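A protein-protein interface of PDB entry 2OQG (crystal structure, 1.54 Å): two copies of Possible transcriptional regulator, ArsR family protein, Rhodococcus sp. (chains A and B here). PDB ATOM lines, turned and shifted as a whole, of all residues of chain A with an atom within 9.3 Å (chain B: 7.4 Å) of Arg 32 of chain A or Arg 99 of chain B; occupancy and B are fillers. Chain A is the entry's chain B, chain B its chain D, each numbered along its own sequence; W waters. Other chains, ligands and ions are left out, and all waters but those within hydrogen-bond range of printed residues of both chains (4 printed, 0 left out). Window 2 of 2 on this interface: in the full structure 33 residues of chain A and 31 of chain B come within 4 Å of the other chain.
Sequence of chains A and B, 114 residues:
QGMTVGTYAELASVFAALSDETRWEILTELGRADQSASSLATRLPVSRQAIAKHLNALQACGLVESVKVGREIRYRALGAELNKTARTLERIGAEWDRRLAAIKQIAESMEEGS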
ATOM      1  N   TRP A  24     -11.954   0.469  11.315  1.00  0.00           N
ATOM      2  CA  TRP A  24     -11.265   1.738  11.057  1.00  0.00           C
ATOM      3  C   TRP A  24      -9.758   1.564  10.881  1.00  0.00           C
ATOM      4  O   TRP A  24      -9.142   2.227  10.016  1.00  0.00           O
ATOM      5  CB  TRP A  24     -11.568   2.785  12.141  1.00  0.00           C
ATOM      6  CG  TRP A  24     -12.866   3.504  11.895  1.00  0.00           C
ATOM      7  CD1 TRP A  24     -14.064   3.297  12.545  1.00  0.00           C
ATOM      8  CD2 TRP A  24     -13.110   4.526  10.906  1.00  0.00           C
ATOM      9  NE1 TRP A  24     -15.038   4.127  12.009  1.00  0.00           N
ATOM     10  CE2 TRP A  24     -14.475   4.903  11.020  1.00  0.00           C
ATOM     11  CE3 TRP A  24     -12.308   5.140   9.928  1.00  0.00           C
ATOM     12  CZ2 TRP A  24     -15.052   5.899  10.200  1.00  0.00           C
ATOM     13  CZ3 TRP A  24     -12.884   6.103   9.086  1.00  0.00           C
ATOM     14  CH2 TRP A  24     -14.231   6.492   9.256  1.00  0.00           C
ATOM     15  N   GLU A  25      -9.168   0.708  11.717  1.00  0.00           N
ATOM     16  CA  GLU A  25      -7.740   0.364  11.645  1.00  0.00           C
ATOM     17  C   GLU A  25      -7.372  -0.293  10.297  1.00  0.00           C
ATOM     18  O   GLU A  25      -6.334   0.034   9.695  1.00  0.00           O
ATOM     19  CB  GLU A  25      -7.345  -0.524  12.839  1.00  0.00           C
ATOM     20  CG  GLU A  25      -7.668   0.084  14.223  1.00  0.00           C
ATOM     21  CD  GLU A  25      -7.240  -0.785  15.429  1.00  0.00           C
ATOM     22  OE1 GLU A  25      -6.084  -1.242  15.449  1.00  0.00           O
ATOM     23  OE2 GLU A  25      -8.051  -0.967  16.385  1.00  0.00           O
ATOM     24  N   ILE A  26      -8.230  -1.204   9.839  1.00  0.00           N
ATOM     25  CA  ILE A  26      -8.067  -1.888   8.543  1.00  0.00           C
ATOM     26  C   ILE A  26      -8.227  -0.862   7.416  1.00  0.00           C
ATOM     27  O   ILE A  26      -7.432  -0.843   6.494  1.00  0.00           O
ATOM     28  CB  ILE A  26      -9.059  -3.067   8.389  1.00  0.00           C
ATOM     29  CG1 ILE A  26      -8.698  -4.230   9.315  1.00  0.00           C
ATOM     30  CG2 ILE A  26      -9.169  -3.528   6.937  1.00  0.00           C
ATOM     31  CD1 ILE A  26      -9.828  -5.224   9.452  1.00  0.00           C
ATOM     32  N   LEU A  27      -9.240   0.009   7.499  1.00  0.00           N
ATOM     33  CA  LEU A  27      -9.415   1.033   6.487  1.00  0.00           C
ATOM     34  C   LEU A  27      -8.224   1.994   6.413  1.00  0.00           C
ATOM     35  O   LEU A  27      -7.756   2.340   5.327  1.00  0.00           O
ATOM     36  CB  LEU A  27     -10.743   1.791   6.726  1.00  0.00           C
ATOM     37  CG  LEU A  27     -12.047   1.097   6.336  1.00  0.00           C
ATOM     38  CD1 LEU A  27     -13.220   1.962   6.906  1.00  0.00           C
ATOM     39  CD2 LEU A  27     -12.220   0.860   4.817  1.00  0.00           C
ATOM     40  N   THR A  28      -7.692   2.401   7.556  1.00  0.00           N
ATOM     41  CA  THR A  28      -6.532   3.298   7.572  1.00  0.00           C
ATOM     42  C   THR A  28      -5.325   2.669   6.862  1.00  0.00           C
ATOM     43  O   THR A  28      -4.645   3.325   6.082  1.00  0.00           O
ATOM     44  CB  THR A  28      -6.226   3.689   9.024  1.00  0.00           C
ATOM     45  OG1 THR A  28      -7.346   4.437   9.492  1.00  0.00           O
ATOM     46  CG2 THR A  28      -4.959   4.559   9.129  1.00  0.00           C
ATOM     47  N   GLU A  29      -5.065   1.402   7.140  1.00  0.00           N
ATOM     48  CA  GLU A  29      -3.972   0.711   6.464  1.00  0.00           C
ATOM     49  C   GLU A  29      -4.198   0.657   4.950  1.00  0.00           C
ATOM     50  O   GLU A  29      -3.274   0.925   4.159  1.00  0.00           O
ATOM     51  CB  GLU A  29      -3.820  -0.690   7.041  1.00  0.00           C
ATOM     52  CG  GLU A  29      -3.026  -0.711   8.331  1.00  0.00           C
ATOM     53  CD  GLU A  29      -1.595  -0.216   8.144  1.00  0.00           C
ATOM     54  OE1 GLU A  29      -0.998  -0.452   7.067  1.00  0.00           O
ATOM     55  OE2 GLU A  29      -1.066   0.396   9.090  1.00  0.00           O
ATOM     56  N   LEU A  30      -5.428   0.326   4.557  1.00  0.00           N
ATOM     57  CA  LEU A  30      -5.765   0.129   3.125  1.00  0.00           C
ATOM     58  C   LEU A  30      -5.918   1.424   2.370  1.00  0.00           C
ATOM     59  O   LEU A  30      -5.927   1.428   1.133  1.00  0.00           O
ATOM     60  CB  LEU A  30      -7.012  -0.717   2.973  1.00  0.00           C
ATOM     61  CG  LEU A  30      -6.973  -2.161   3.461  1.00  0.00           C
ATOM     62  CD1 LEU A  30      -8.337  -2.774   3.330  1.00  0.00           C
ATOM     63  CD2 LEU A  30      -5.867  -2.999   2.765  1.00  0.00           C
ATOM     64  N   GLY A  31      -6.074   2.527   3.107  1.00  0.00           N
ATOM     65  CA  GLY A  31      -6.044   3.820   2.463  1.00  0.00           C
ATOM     66  C   GLY A  31      -4.647   4.347   2.172  1.00  0.00           C
ATOM     67  O   GLY A  31      -4.505   5.218   1.332  1.00  0.00           O
ATOM     68  N   ARG A  32      -3.636   3.824   2.873  1.00  0.00           N
ATOM     69  CA  ARG A  32      -2.232   4.220   2.667  1.00  0.00           C
ATOM     70  C   ARG A  32      -1.501   3.323   1.654  1.00  0.00           C
ATOM     71  O   ARG A  32      -0.577   3.772   0.968  1.00  0.00           O
ATOM     72  CB  ARG A  32      -1.452   4.217   3.983  1.00  0.00           C
ATOM     73  CG  ARG A  32      -1.724   5.421   4.887  1.00  0.00           C
ATOM     74  CD  ARG A  32      -0.799   5.440   6.105  1.00  0.00           C
ATOM     75  NE  ARG A  32       0.589   5.784   5.774  1.00  0.00           N
ATOM     76  CZ  ARG A  32       1.085   7.019   5.763  1.00  0.00           C
ATOM     77  NH1 ARG A  32       2.362   7.211   5.452  1.00  0.00           N
ATOM     78  NH2 ARG A  32       0.313   8.057   6.069  1.00  0.00           N
ATOM     79  N   ALA A  33      -1.903   2.055   1.585  1.00  0.00           N
ATOM     80  CA  ALA A  33      -1.296   1.084   0.656  1.00  0.00           C
ATOM     81  C   ALA A  33      -2.255  -0.065   0.379  1.00  0.00           C
ATOM     82  O   ALA A  33      -2.849  -0.611   1.302  1.00  0.00           O
ATOM     83  CB  ALA A  33       0.016   0.543   1.235  1.00  0.00           C
ATOM     84  N   ASP A  34      -2.360  -0.498  -0.879  1.00  0.00           N
ATOM     85  CA  ASP A  34      -3.161  -1.688  -1.211  1.00  0.00           C
ATOM     86  C   ASP A  34      -2.481  -2.863  -0.503  1.00  0.00           C
ATOM     87  O   ASP A  34      -1.265  -3.014  -0.633  1.00  0.00           O
ATOM     88  CB  ASP A  34      -3.084  -2.028  -2.715  1.00  0.00           C
ATOM     89  CG  ASP A  34      -3.779  -1.037  -3.641  1.00  0.00           C
ATOM     90  OD1 ASP A  34      -4.383  -0.003  -3.189  1.00  0.00           O
ATOM     91  OD2 ASP A  34      -3.706  -1.330  -4.892  1.00  0.00           O
ATOM     92  N   GLN A  35      -3.212  -3.691   0.220  1.00  0.00           N
ATOM     93  CA  GLN A  35      -2.554  -4.777   0.989  1.00  0.00           C
ATOM     94  C   GLN A  35      -3.357  -6.049   0.926  1.00  0.00           C
ATOM     95  O   GLN A  35      -4.576  -6.014   0.845  1.00  0.00           O
ATOM     96  CB  GLN A  35      -2.413  -4.369   2.465  1.00  0.00           C
ATOM     97  CG  GLN A  35      -1.392  -3.275   2.690  1.00  0.00           C
ATOM     98  CD  GLN A  35      -1.233  -2.955   4.141  1.00  0.00           C
ATOM     99  OE1 GLN A  35      -0.911  -3.834   4.955  1.00  0.00           O
ATOM    100  NE2 GLN A  35      -1.467  -1.698   4.494  1.00  0.00           N
ATOM    101  N   LEU A  40      -2.157  -7.405   6.120  1.00  0.00           N
ATOM    102  CA  LEU A  40      -2.939  -6.833   7.240  1.00  0.00           C
ATOM    103  C   LEU A  40      -2.712  -7.631   8.537  1.00  0.00           C
ATOM    104  O   LEU A  40      -2.537  -7.042   9.598  1.00  0.00           O
ATOM    105  CB  LEU A  40      -4.430  -6.812   6.901  1.00  0.00           C
ATOM    106  CG  LEU A  40      -4.829  -5.773   5.853  1.00  0.00           C
ATOM    107  CD1 LEU A  40      -6.287  -5.998   5.467  1.00  0.00           C
ATOM    108  CD2 LEU A  40      -4.626  -4.362   6.394  1.00  0.00           C
ATOM    109  N   ARG A  43       0.420  -6.879  10.126  1.00  0.00           N
ATOM    110  CA  ARG A  43       0.481  -5.510  10.625  1.00  0.00           C
ATOM    111  C   ARG A  43      -0.372  -5.286  11.873  1.00  0.00           C
ATOM    112  O   ARG A  43       0.014  -4.521  12.751  1.00  0.00           O
ATOM    113  CB  ARG A  43       0.104  -4.531   9.508  1.00  0.00           C
ATOM    114  CG  ARG A  43       0.067  -3.077   9.930  1.00  0.00           C
ATOM    115  CD  ARG A  43       0.943  -2.221   9.027  1.00  0.00           C
ATOM    116  NE  ARG A  43       2.328  -2.168   9.501  1.00  0.00           N
ATOM    117  CZ  ARG A  43       2.762  -1.401  10.503  1.00  0.00           C
ATOM    118  NH1 ARG A  43       4.040  -1.434  10.843  1.00  0.00           N
ATOM    119  NH2 ARG A  43       1.926  -0.607  11.169  1.00  0.00           N
ATOM    120  N   VAL A  64     -14.347  -0.770   0.531  1.00  0.00           N
ATOM    121  CA  VAL A  64     -13.100  -1.376   0.058  1.00  0.00           C
ATOM    122  C   VAL A  64     -13.381  -2.106  -1.251  1.00  0.00           C
ATOM    123  O   VAL A  64     -14.459  -2.624  -1.445  1.00  0.00           O
ATOM    124  CB  VAL A  64     -12.559  -2.366   1.159  1.00  0.00           C
ATOM    125  CG1 VAL A  64     -11.549  -3.318   0.609  1.00  0.00           C
ATOM    126  CG2 VAL A  64     -12.028  -1.549   2.353  1.00  0.00           C
ATOM    127  N   GLU A  65     -12.394  -2.161  -2.130  1.00  0.00           N
ATOM    128  CA  GLU A  65     -12.492  -3.006  -3.331  1.00  0.00           C
ATOM    129  C   GLU A  65     -11.264  -3.910  -3.357  1.00  0.00           C
ATOM    130  O   GLU A  65     -10.174  -3.545  -2.886  1.00  0.00           O
ATOM    131  CB  GLU A  65     -12.494  -2.167  -4.630  1.00  0.00           C
ATOM    132  CG  GLU A  65     -11.196  -1.353  -4.870  1.00  0.00           C
ATOM    133  CD  GLU A  65     -11.321  -0.421  -6.098  1.00  0.00           C
ATOM    134  OE1 GLU A  65     -12.359  -0.516  -6.800  1.00  0.00           O
ATOM    135  OE2 GLU A  65     -10.400   0.418  -6.386  1.00  0.00           O
ATOM    136  N   VAL A  67      -8.264  -5.771  -5.418  1.00  0.00           N
ATOM    137  CA  VAL A  67      -7.388  -5.432  -6.520  1.00  0.00           C
ATOM    138  C   VAL A  67      -6.622  -6.734  -6.801  1.00  0.00           C
ATOM    139  O   VAL A  67      -5.809  -7.187  -5.974  1.00  0.00           O
ATOM    140  CB  VAL A  67      -6.392  -4.298  -6.161  1.00  0.00           C
ATOM    141  CG1 VAL A  67      -5.448  -4.000  -7.324  1.00  0.00           C
ATOM    142  CG2 VAL A  67      -7.103  -3.018  -5.677  1.00  0.00           C
ATOM    143  N   ARG A  74      -5.209  -8.113  -3.346  1.00  0.00           N
ATOM    144  CA  ARG A  74      -5.037  -7.033  -2.386  1.00  0.00           C
ATOM    145  C   ARG A  74      -6.357  -6.288  -2.230  1.00  0.00           C
ATOM    146  O   ARG A  74      -7.341  -6.575  -2.933  1.00  0.00           O
ATOM    147  CB  ARG A  74      -3.918  -6.099  -2.845  1.00  0.00           C
ATOM    148  CG  ARG A  74      -2.527  -6.791  -2.956  1.00  0.00           C
ATOM    149  CD  ARG A  74      -1.405  -5.763  -3.218  1.00  0.00           C
ATOM    150  NE  ARG A  74      -0.067  -6.359  -3.234  1.00  0.00           N
ATOM    151  CZ  ARG A  74       0.476  -6.954  -4.295  1.00  0.00           C
ATOM    152  NH1 ARG A  74       1.695  -7.474  -4.214  1.00  0.00           N
ATOM    153  NH2 ARG A  74      -0.201  -7.027  -5.443  1.00  0.00           N
ATOM    154  N   TYR A  75      -6.376  -5.365  -1.275  1.00  0.00           N
ATOM    155  CA  TYR A  75      -7.559  -4.539  -1.009  1.00  0.00           C
ATOM    156  C   TYR A  75      -7.199  -3.053  -0.941  1.00  0.00           C
ATOM    157  O   TYR A  75      -6.107  -2.691  -0.605  1.00  0.00           O
ATOM    158  CB  TYR A  75      -8.239  -5.010   0.291  1.00  0.00           C
ATOM    159  CG  TYR A  75      -8.696  -6.463   0.157  1.00  0.00           C
ATOM    160  CD1 TYR A  75      -9.948  -6.767  -0.325  1.00  0.00           C
ATOM    161  CD2 TYR A  75      -7.829  -7.534   0.481  1.00  0.00           C
ATOM    162  CE1 TYR A  75     -10.376  -8.092  -0.497  1.00  0.00           C
ATOM    163  CE2 TYR A  75      -8.231  -8.855   0.331  1.00  0.00           C
ATOM    164  CZ  TYR A  75      -9.504  -9.131  -0.170  1.00  0.00           C
ATOM    165  OH  TYR A  75      -9.892 -10.440  -0.337  1.00  0.00           O
ATOM    166  N   ARG A  76      -8.168  -2.213  -1.265  1.00  0.00           N
ATOM    167  CA  ARG A  76      -7.927  -0.778  -1.317  1.00  0.00           C
ATOM    168  C   ARG A  76      -9.118  -0.070  -0.675  1.00  0.00           C
ATOM    169  O   ARG A  76     -10.248  -0.404  -0.988  1.00  0.00           O
ATOM    170  CB  ARG A  76      -7.812  -0.367  -2.779  1.00  0.00           C
ATOM    171  CG  ARG A  76      -7.605   1.119  -2.967  1.00  0.00           C
ATOM    172  CD  ARG A  76      -7.505   1.473  -4.442  1.00  0.00           C
ATOM    173  NE  ARG A  76      -6.316   0.856  -5.039  1.00  0.00           N
ATOM    174  CZ  ARG A  76      -6.214   0.545  -6.334  1.00  0.00           C
ATOM    175  NH1 ARG A  76      -7.250   0.792  -7.163  1.00  0.00           N
ATOM    176  NH2 ARG A  76      -5.076   0.031  -6.799  1.00  0.00           N
ATOM    177  N   ALA A  77      -8.856   0.887   0.210  1.00  0.00           N
ATOM    178  CA  ALA A  77      -9.952   1.691   0.757  1.00  0.00           C
ATOM    179  C   ALA A  77     -10.362   2.730  -0.249  1.00  0.00           C
ATOM    180  O   ALA A  77      -9.513   3.361  -0.882  1.00  0.00           O
ATOM    181  CB  ALA A  77      -9.541   2.342   2.031  1.00  0.00           C
ATOM    182  N   LEU A  78     -11.667   2.939  -0.351  1.00  0.00           N
ATOM    183  CA  LEU A  78     -12.217   3.933  -1.267  1.00  0.00           C
ATOM    184  C   LEU A  78     -12.934   5.057  -0.509  1.00  0.00           C
ATOM    185  O   LEU A  78     -13.735   4.830   0.419  1.00  0.00           O
ATOM    186  CB  LEU A  78     -13.230   3.307  -2.196  1.00  0.00           C
ATOM    187  CG  LEU A  78     -12.646   2.175  -3.058  1.00  0.00           C
ATOM    188  CD1 LEU A  78     -13.812   1.371  -3.655  1.00  0.00           C
ATOM    189  CD2 LEU A  78     -11.718   2.735  -4.124  1.00  0.00           C
ATOM    190  N   GLY A  79     -12.648   6.285  -0.912  1.00  0.00           N
ATOM    191  CA  GLY A  79     -13.244   7.432  -0.224  1.00  0.00           C
ATOM    192  C   GLY A  79     -14.694   7.675  -0.548  1.00  0.00           C
ATOM    193  O   GLY A  79     -15.387   8.355   0.222  1.00  0.00           O
ATOM    194  N   GLY B  93     -11.351  10.819   3.492  1.00  0.00           N
ATOM    195  CA  GLY B  93     -11.795  10.561   2.147  1.00  0.00           C
ATOM    196  C   GLY B  93     -10.864  11.216   1.154  1.00  0.00           C
ATOM    197  O   GLY B  93     -10.415  10.558   0.202  1.00  0.00           O
ATOM    198  N   ALA B  94     -10.543  12.492   1.391  1.00  0.00           N
ATOM    199  CA  ALA B  94      -9.607  13.242   0.528  1.00  0.00           C
ATOM    200  C   ALA B  94      -8.252  12.550   0.379  1.00  0.00           C
ATOM    201  O   ALA B  94      -7.685  12.544  -0.706  1.00  0.00           O
ATOM    202  CB  ALA B  94      -9.401  14.669   1.078  1.00  0.00           C
ATOM    203  N   GLU B  95      -7.737  11.982   1.468  1.00  0.00           N
ATOM    204  CA  GLU B  95      -6.427  11.324   1.449  1.00  0.00           C
ATOM    205  C   GLU B  95      -6.455  10.000   0.672  1.00  0.00           C
ATOM    206  O   GLU B  95      -5.460   9.618   0.058  1.00  0.00           O
ATOM    207  CB  GLU B  95      -5.926  11.051   2.866  1.00  0.00           C
ATOM    208  CG  GLU B  95      -5.827  12.267   3.759  1.00  0.00           C
ATOM    209  CD  GLU B  95      -5.979  11.909   5.225  1.00  0.00           C
ATOM    210  OE1 GLU B  95      -5.825  10.711   5.583  1.00  0.00           O
ATOM    211  OE2 GLU B  95      -6.257  12.825   6.029  1.00  0.00           O
ATOM    212  N   TRP B  96      -7.587   9.311   0.715  1.00  0.00           N
ATOM    213  CA  TRP B  96      -7.791   8.088  -0.098  1.00  0.00           C
ATOM    214  C   TRP B  96      -8.042   8.397  -1.577  1.00  0.00           C
ATOM    215  O   TRP B  96      -7.477   7.715  -2.454  1.00  0.00           O
ATOM    216  CB  TRP B  96      -8.909   7.205   0.438  1.00  0.00           C
ATOM    217  CG  TRP B  96      -8.776   6.764   1.850  1.00  0.00           C
ATOM    218  CD1 TRP B  96      -7.670   6.860   2.673  1.00  0.00           C
ATOM    219  CD2 TRP B  96      -9.780   6.104   2.606  1.00  0.00           C
ATOM    220  NE1 TRP B  96      -7.955   6.323   3.908  1.00  0.00           N
ATOM    221  CE2 TRP B  96      -9.242   5.849   3.886  1.00  0.00           C
ATOM    222  CE3 TRP B  96     -11.097   5.713   2.323  1.00  0.00           C
ATOM    223  CZ2 TRP B  96      -9.973   5.208   4.896  1.00  0.00           C
ATOM    224  CZ3 TRP B  96     -11.842   5.067   3.343  1.00  0.00           C
ATOM    225  CH2 TRP B  96     -11.265   4.826   4.599  1.00  0.00           C
ATOM    226  N   ASP B  97      -8.848   9.436  -1.856  1.00  0.00           N
ATOM    227  CA  ASP B  97      -9.061   9.923  -3.223  1.00  0.00           C
ATOM    228  C   ASP B  97      -7.769  10.399  -3.918  1.00  0.00           C
ATOM    229  O   ASP B  97      -7.592  10.158  -5.123  1.00  0.00           O
ATOM    230  CB  ASP B  97     -10.072  11.064  -3.214  1.00  0.00           C
ATOM    231  CG  ASP B  97     -11.493  10.591  -2.937  1.00  0.00           C
ATOM    232  OD1 ASP B  97     -11.751   9.357  -2.842  1.00  0.00           O
ATOM    233  OD2 ASP B  97     -12.353  11.475  -2.774  1.00  0.00           O
ATOM    234  N   ARG B  98      -6.864  11.052  -3.176  1.00  0.00           N
ATOM    235  CA  ARG B  98      -5.565  11.480  -3.744  1.00  0.00           C
ATOM    236  C   ARG B  98      -4.668  10.285  -4.120  1.00  0.00           C
ATOM    237  O   ARG B  98      -4.004  10.298  -5.166  1.00  0.00           O
ATOM    238  CB  ARG B  98      -4.782  12.395  -2.793  1.00  0.00           C
ATOM    239  CG  ARG B  98      -5.322  13.821  -2.607  1.00  0.00           C
ATOM    240  CD  ARG B  98      -4.262  14.688  -1.913  1.00  0.00           C
ATOM    241  NE  ARG B  98      -4.047  14.376  -0.499  1.00  0.00           N
ATOM    242  CZ  ARG B  98      -4.748  14.911   0.497  1.00  0.00           C
ATOM    243  NH1 ARG B  98      -5.700  15.795   0.235  1.00  0.00           N
ATOM    244  NH2 ARG B  98      -4.494  14.579   1.757  1.00  0.00           N
ATOM    245  N   ARG B  99      -4.613   9.272  -3.262  1.00  0.00           N
ATOM    246  CA  ARG B  99      -3.839   8.079  -3.607  1.00  0.00           C
ATOM    247  C   ARG B  99      -4.458   7.384  -4.838  1.00  0.00           C
ATOM    248  O   ARG B  99      -3.732   6.946  -5.751  1.00  0.00           O
ATOM    249  CB  ARG B  99      -3.680   7.127  -2.411  1.00  0.00           C
ATOM    250  CG  ARG B  99      -2.709   5.959  -2.707  1.00  0.00           C
ATOM    251  CD  ARG B  99      -2.387   5.132  -1.466  1.00  0.00           C
ATOM    252  NE  ARG B  99      -3.403   4.134  -1.132  1.00  0.00           N
ATOM    253  CZ  ARG B  99      -3.458   2.914  -1.652  1.00  0.00           C
ATOM    254  NH1 ARG B  99      -2.598   2.565  -2.608  1.00  0.00           N
ATOM    255  NH2 ARG B  99      -4.414   2.062  -1.273  1.00  0.00           N
ATOM    256  N   LEU B 100      -5.796   7.317  -4.878  1.00  0.00           N
ATOM    257  CA  LEU B 100      -6.472   6.728  -6.020  1.00  0.00           C
ATOM    258  C   LEU B 100      -6.183   7.442  -7.312  1.00  0.00           C
ATOM    259  O   LEU B 100      -5.922   6.810  -8.356  1.00  0.00           O
ATOM    260  CB  LEU B 100      -7.979   6.644  -5.835  1.00  0.00           C
ATOM    261  CG  LEU B 100      -8.758   5.795  -6.869  1.00  0.00           C
ATOM    262  CD1 LEU B 100      -8.276   4.300  -7.008  1.00  0.00           C
ATOM    263  CD2 LEU B 100     -10.237   5.838  -6.601  1.00  0.00           C
ATOM    264  N   ALA B 101      -6.315   8.762  -7.269  1.00  0.00           N
ATOM    265  CA  ALA B 101      -6.011   9.553  -8.440  1.00  0.00           C
ATOM    266  C   ALA B 101      -4.588   9.350  -8.930  1.00  0.00           C
ATOM    267  O   ALA B 101      -4.366   9.208 -10.123  1.00  0.00           O
ATOM    268  CB  ALA B 101      -6.270  11.024  -8.159  1.00  0.00           C
ATOM    269  N   ALA B 102      -3.636   9.354  -8.002  1.00  0.00           N
ATOM    270  CA  ALA B 102      -2.239   9.145  -8.353  1.00  0.00           C
ATOM    271  C   ALA B 102      -2.043   7.792  -9.059  1.00  0.00           C
ATOM    272  O   ALA B 102      -1.315   7.737 -10.074  1.00  0.00           O
ATOM    273  CB  ALA B 102      -1.342   9.258  -7.141  1.00  0.00           C
ATOM    274  N   ILE B 103      -2.625   6.723  -8.498  1.00  0.00           N
ATOM    275  CA  ILE B 103      -2.478   5.386  -9.093  1.00  0.00           C
ATOM    276  C   ILE B 103      -3.029   5.464 -10.505  1.00  0.00           C
ATOM    277  O   ILE B 103      -2.377   5.096 -11.493  1.00  0.00           O
ATOM    278  CB  ILE B 103      -3.270   4.288  -8.327  1.00  0.00           C
ATOM    279  CG1 ILE B 103      -2.695   4.107  -6.913  1.00  0.00           C
ATOM    280  CG2 ILE B 103      -3.217   2.957  -9.112  1.00  0.00           C
ATOM    281  CD1 ILE B 103      -3.557   3.319  -5.976  1.00  0.00           C
ATOM    282  N   LYS B 104      -4.253   5.987 -10.602  1.00  0.00           N
ATOM    283  CA  LYS B 104      -4.956   6.151 -11.878  1.00  0.00           C
ATOM    284  C   LYS B 104      -4.147   6.938 -12.915  1.00  0.00           C
ATOM    285  O   LYS B 104      -4.091   6.539 -14.068  1.00  0.00           O
ATOM    286  CB  LYS B 104      -6.333   6.805 -11.676  1.00  0.00           C
ATOM    287  CG  LYS B 104      -7.421   5.866 -11.117  1.00  0.00           C
ATOM    288  CD  LYS B 104      -8.784   6.575 -11.020  1.00  0.00           C
ATOM    289  CE  LYS B 104      -8.908   7.359  -9.700  1.00  0.00           C
ATOM    290  NZ  LYS B 104      -9.989   8.369  -9.532  1.00  0.00           N
ATOM    291  N   GLN B 105      -3.489   8.028 -12.500  1.00  0.00           N
ATOM    292  CA  GLN B 105      -2.764   8.873 -13.470  1.00  0.00           C
ATOM    293  C   GLN B 105      -1.581   8.156 -14.127  1.00  0.00           C
ATOM    294  O   GLN B 105      -1.080   8.609 -15.174  1.00  0.00           O
ATOM    295  CB  GLN B 105      -2.321  10.216 -12.863  1.00  0.00           C
ATOM    296  CG  GLN B 105      -3.472  11.233 -12.688  1.00  0.00           C
ATOM    297  CD  GLN B 105      -2.990  12.680 -12.454  1.00  0.00           C
ATOM    298  OE1 GLN B 105      -2.139  13.206 -13.188  1.00  0.00           O
ATOM    299  NE2 GLN B 105      -3.571  13.334 -11.454  1.00  0.00           N
HETATM  300  O   HOH W   1     -10.952   6.696  -3.140  1.00  0.00           O
HETATM  301  O   HOH W   2      -8.580   5.051  -2.827  1.00  0.00           O
HETATM  302  O   HOH W   3      -6.858   4.404  -1.062  1.00  0.00           O
HETATM  303  O   HOH W   4      -4.988   5.919   5.645  1.00  0.00           O
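Water W4 lies within hydrogen-bond range of the backbone carbonyl oxygen of Thr 28 of chain A and the indole nitrogen of Trp 96 of chain B.
Water W2 lies within hydrogen-bond range of the backbone carbonyl oxygen of Ala 77 of chain A (2.7 Å) and the backbone carbonyl oxygen of Trp 96 of chain B (2.9 Å).
Water W3 lies within hydrogen-bond range of O of Ala 77 of chain A, NH2 of Arg 99 of chain B and O of Gly 31 of chain A.
No position is printed for both chains.
The backbone carbonyl oxygen of Leu 30 of chain A sits at hydrogen-bond distance from the backbone NH of Ala 77 of chain A.
The side-chain carboxylate of Asp 34 of chain A is in salt-bridge range of the guanidinium group of Arg 76 of chain A, at 2.7 Å.
NH1 of Arg 76 of chain A is in salt-bridge range of OE2 of Glu 65 of chain A (3.3 Å).
Among the printed residues, merely in contact across the chains: Arg 32 of chain A with Arg 99 of chain B (3.3 Å), Leu 78 of chain A with Trp 96 of chain B (3.4 Å), Ala 33 of chain A with Arg 99 of chain B (3.5 Å), Gly 31 of chain A with Trp 96 of chain B (3.5 Å), Gly 79 of chain A with Asp 97 of chain B (3.6 Å), Gly 79 of chain A with Trp 96 of chain B (3.6 Å), Leu 27 of chain A with Trp 96 of chain B (3.7 Å), Arg 76 of chain A with Leu 100 of chain B (3.7 Å), Arg 76 of chain A with Ile 103 of chain B (3.7 Å), Ala 77 of chain A with Trp 96 of chain B (3.7 Å) and Arg 76 of chain A with Arg 99 of chain B (3.7 Å).
The side-chain carboxylate (OD1) of Asp 34 of chain A lies within salt-bridge range of the guanidinium group (NH2) of Arg 99 of chain B, 2.8 Å away.
The backbone carbonyl oxygen (O) of Gly 31 of chain A sits at hydrogen-bond distance from the guanidinium group (NE) of Arg 99 of chain B (2.9 Å).
O of Leu 30 of chain A sits at hydrogen-bond distance from NH2 of Arg 99 of chain B, at 2.9 Å.
Of the 23 printed residues of chain A, 10 touch a printed residue of chain B.
Hydrophobic or aromatic side chains of chain A within 4 Å of the printed part of chain B: Leu 27 and Ala 77.
Along chain A the printed residues that touch a printed residue of chain B span positions 27 to 79.
Printed residues of chain B that touch a printed residue of chain A: Trp 96, Asp 97, Arg 99, Leu 100 and Ile 103.
Among the printed residues, Asp or Glu carboxylates within 4 Å of a Lys or Arg side-chain nitrogen of the other chain: Asp 34 of chain A with Arg 99 of chain B (2.8 Å).
Printed residues of chain B within 4 Å of Arg 32 of chain A: Arg 99 (3.3 Å).
Printed residues of chain A within 4 Å of Arg 99 of chain B: Leu 30 (2.9 Å), Gly 31 (2.9 Å), Arg 32 (3.3 Å), Ala 33 (3.5 Å), Asp 34 (2.8 Å) and Arg 76 (3.7 Å).
No residue of chain A comes within 4 Å of Ala 101 of chain B.
No residue of chain A comes within 4 Å of Ala 102 of chain B.
Printed residues of chain B within 4 Å of Leu 78 of chain A: Trp 96.
Printed residues of chain B within 4 Å of Arg 76 of chain A: Arg 99, Leu 100 and Ile 103.
Printed residues of chain B within 4 Å of Asp 34 of chain A: Arg 99.
Glu 95 of chain B touches none of the printed residues of chain A.
The nearest printed residue of chain B that does not touch Arg 76 of chain A is Lys 104 of chain B (6.4 Å).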
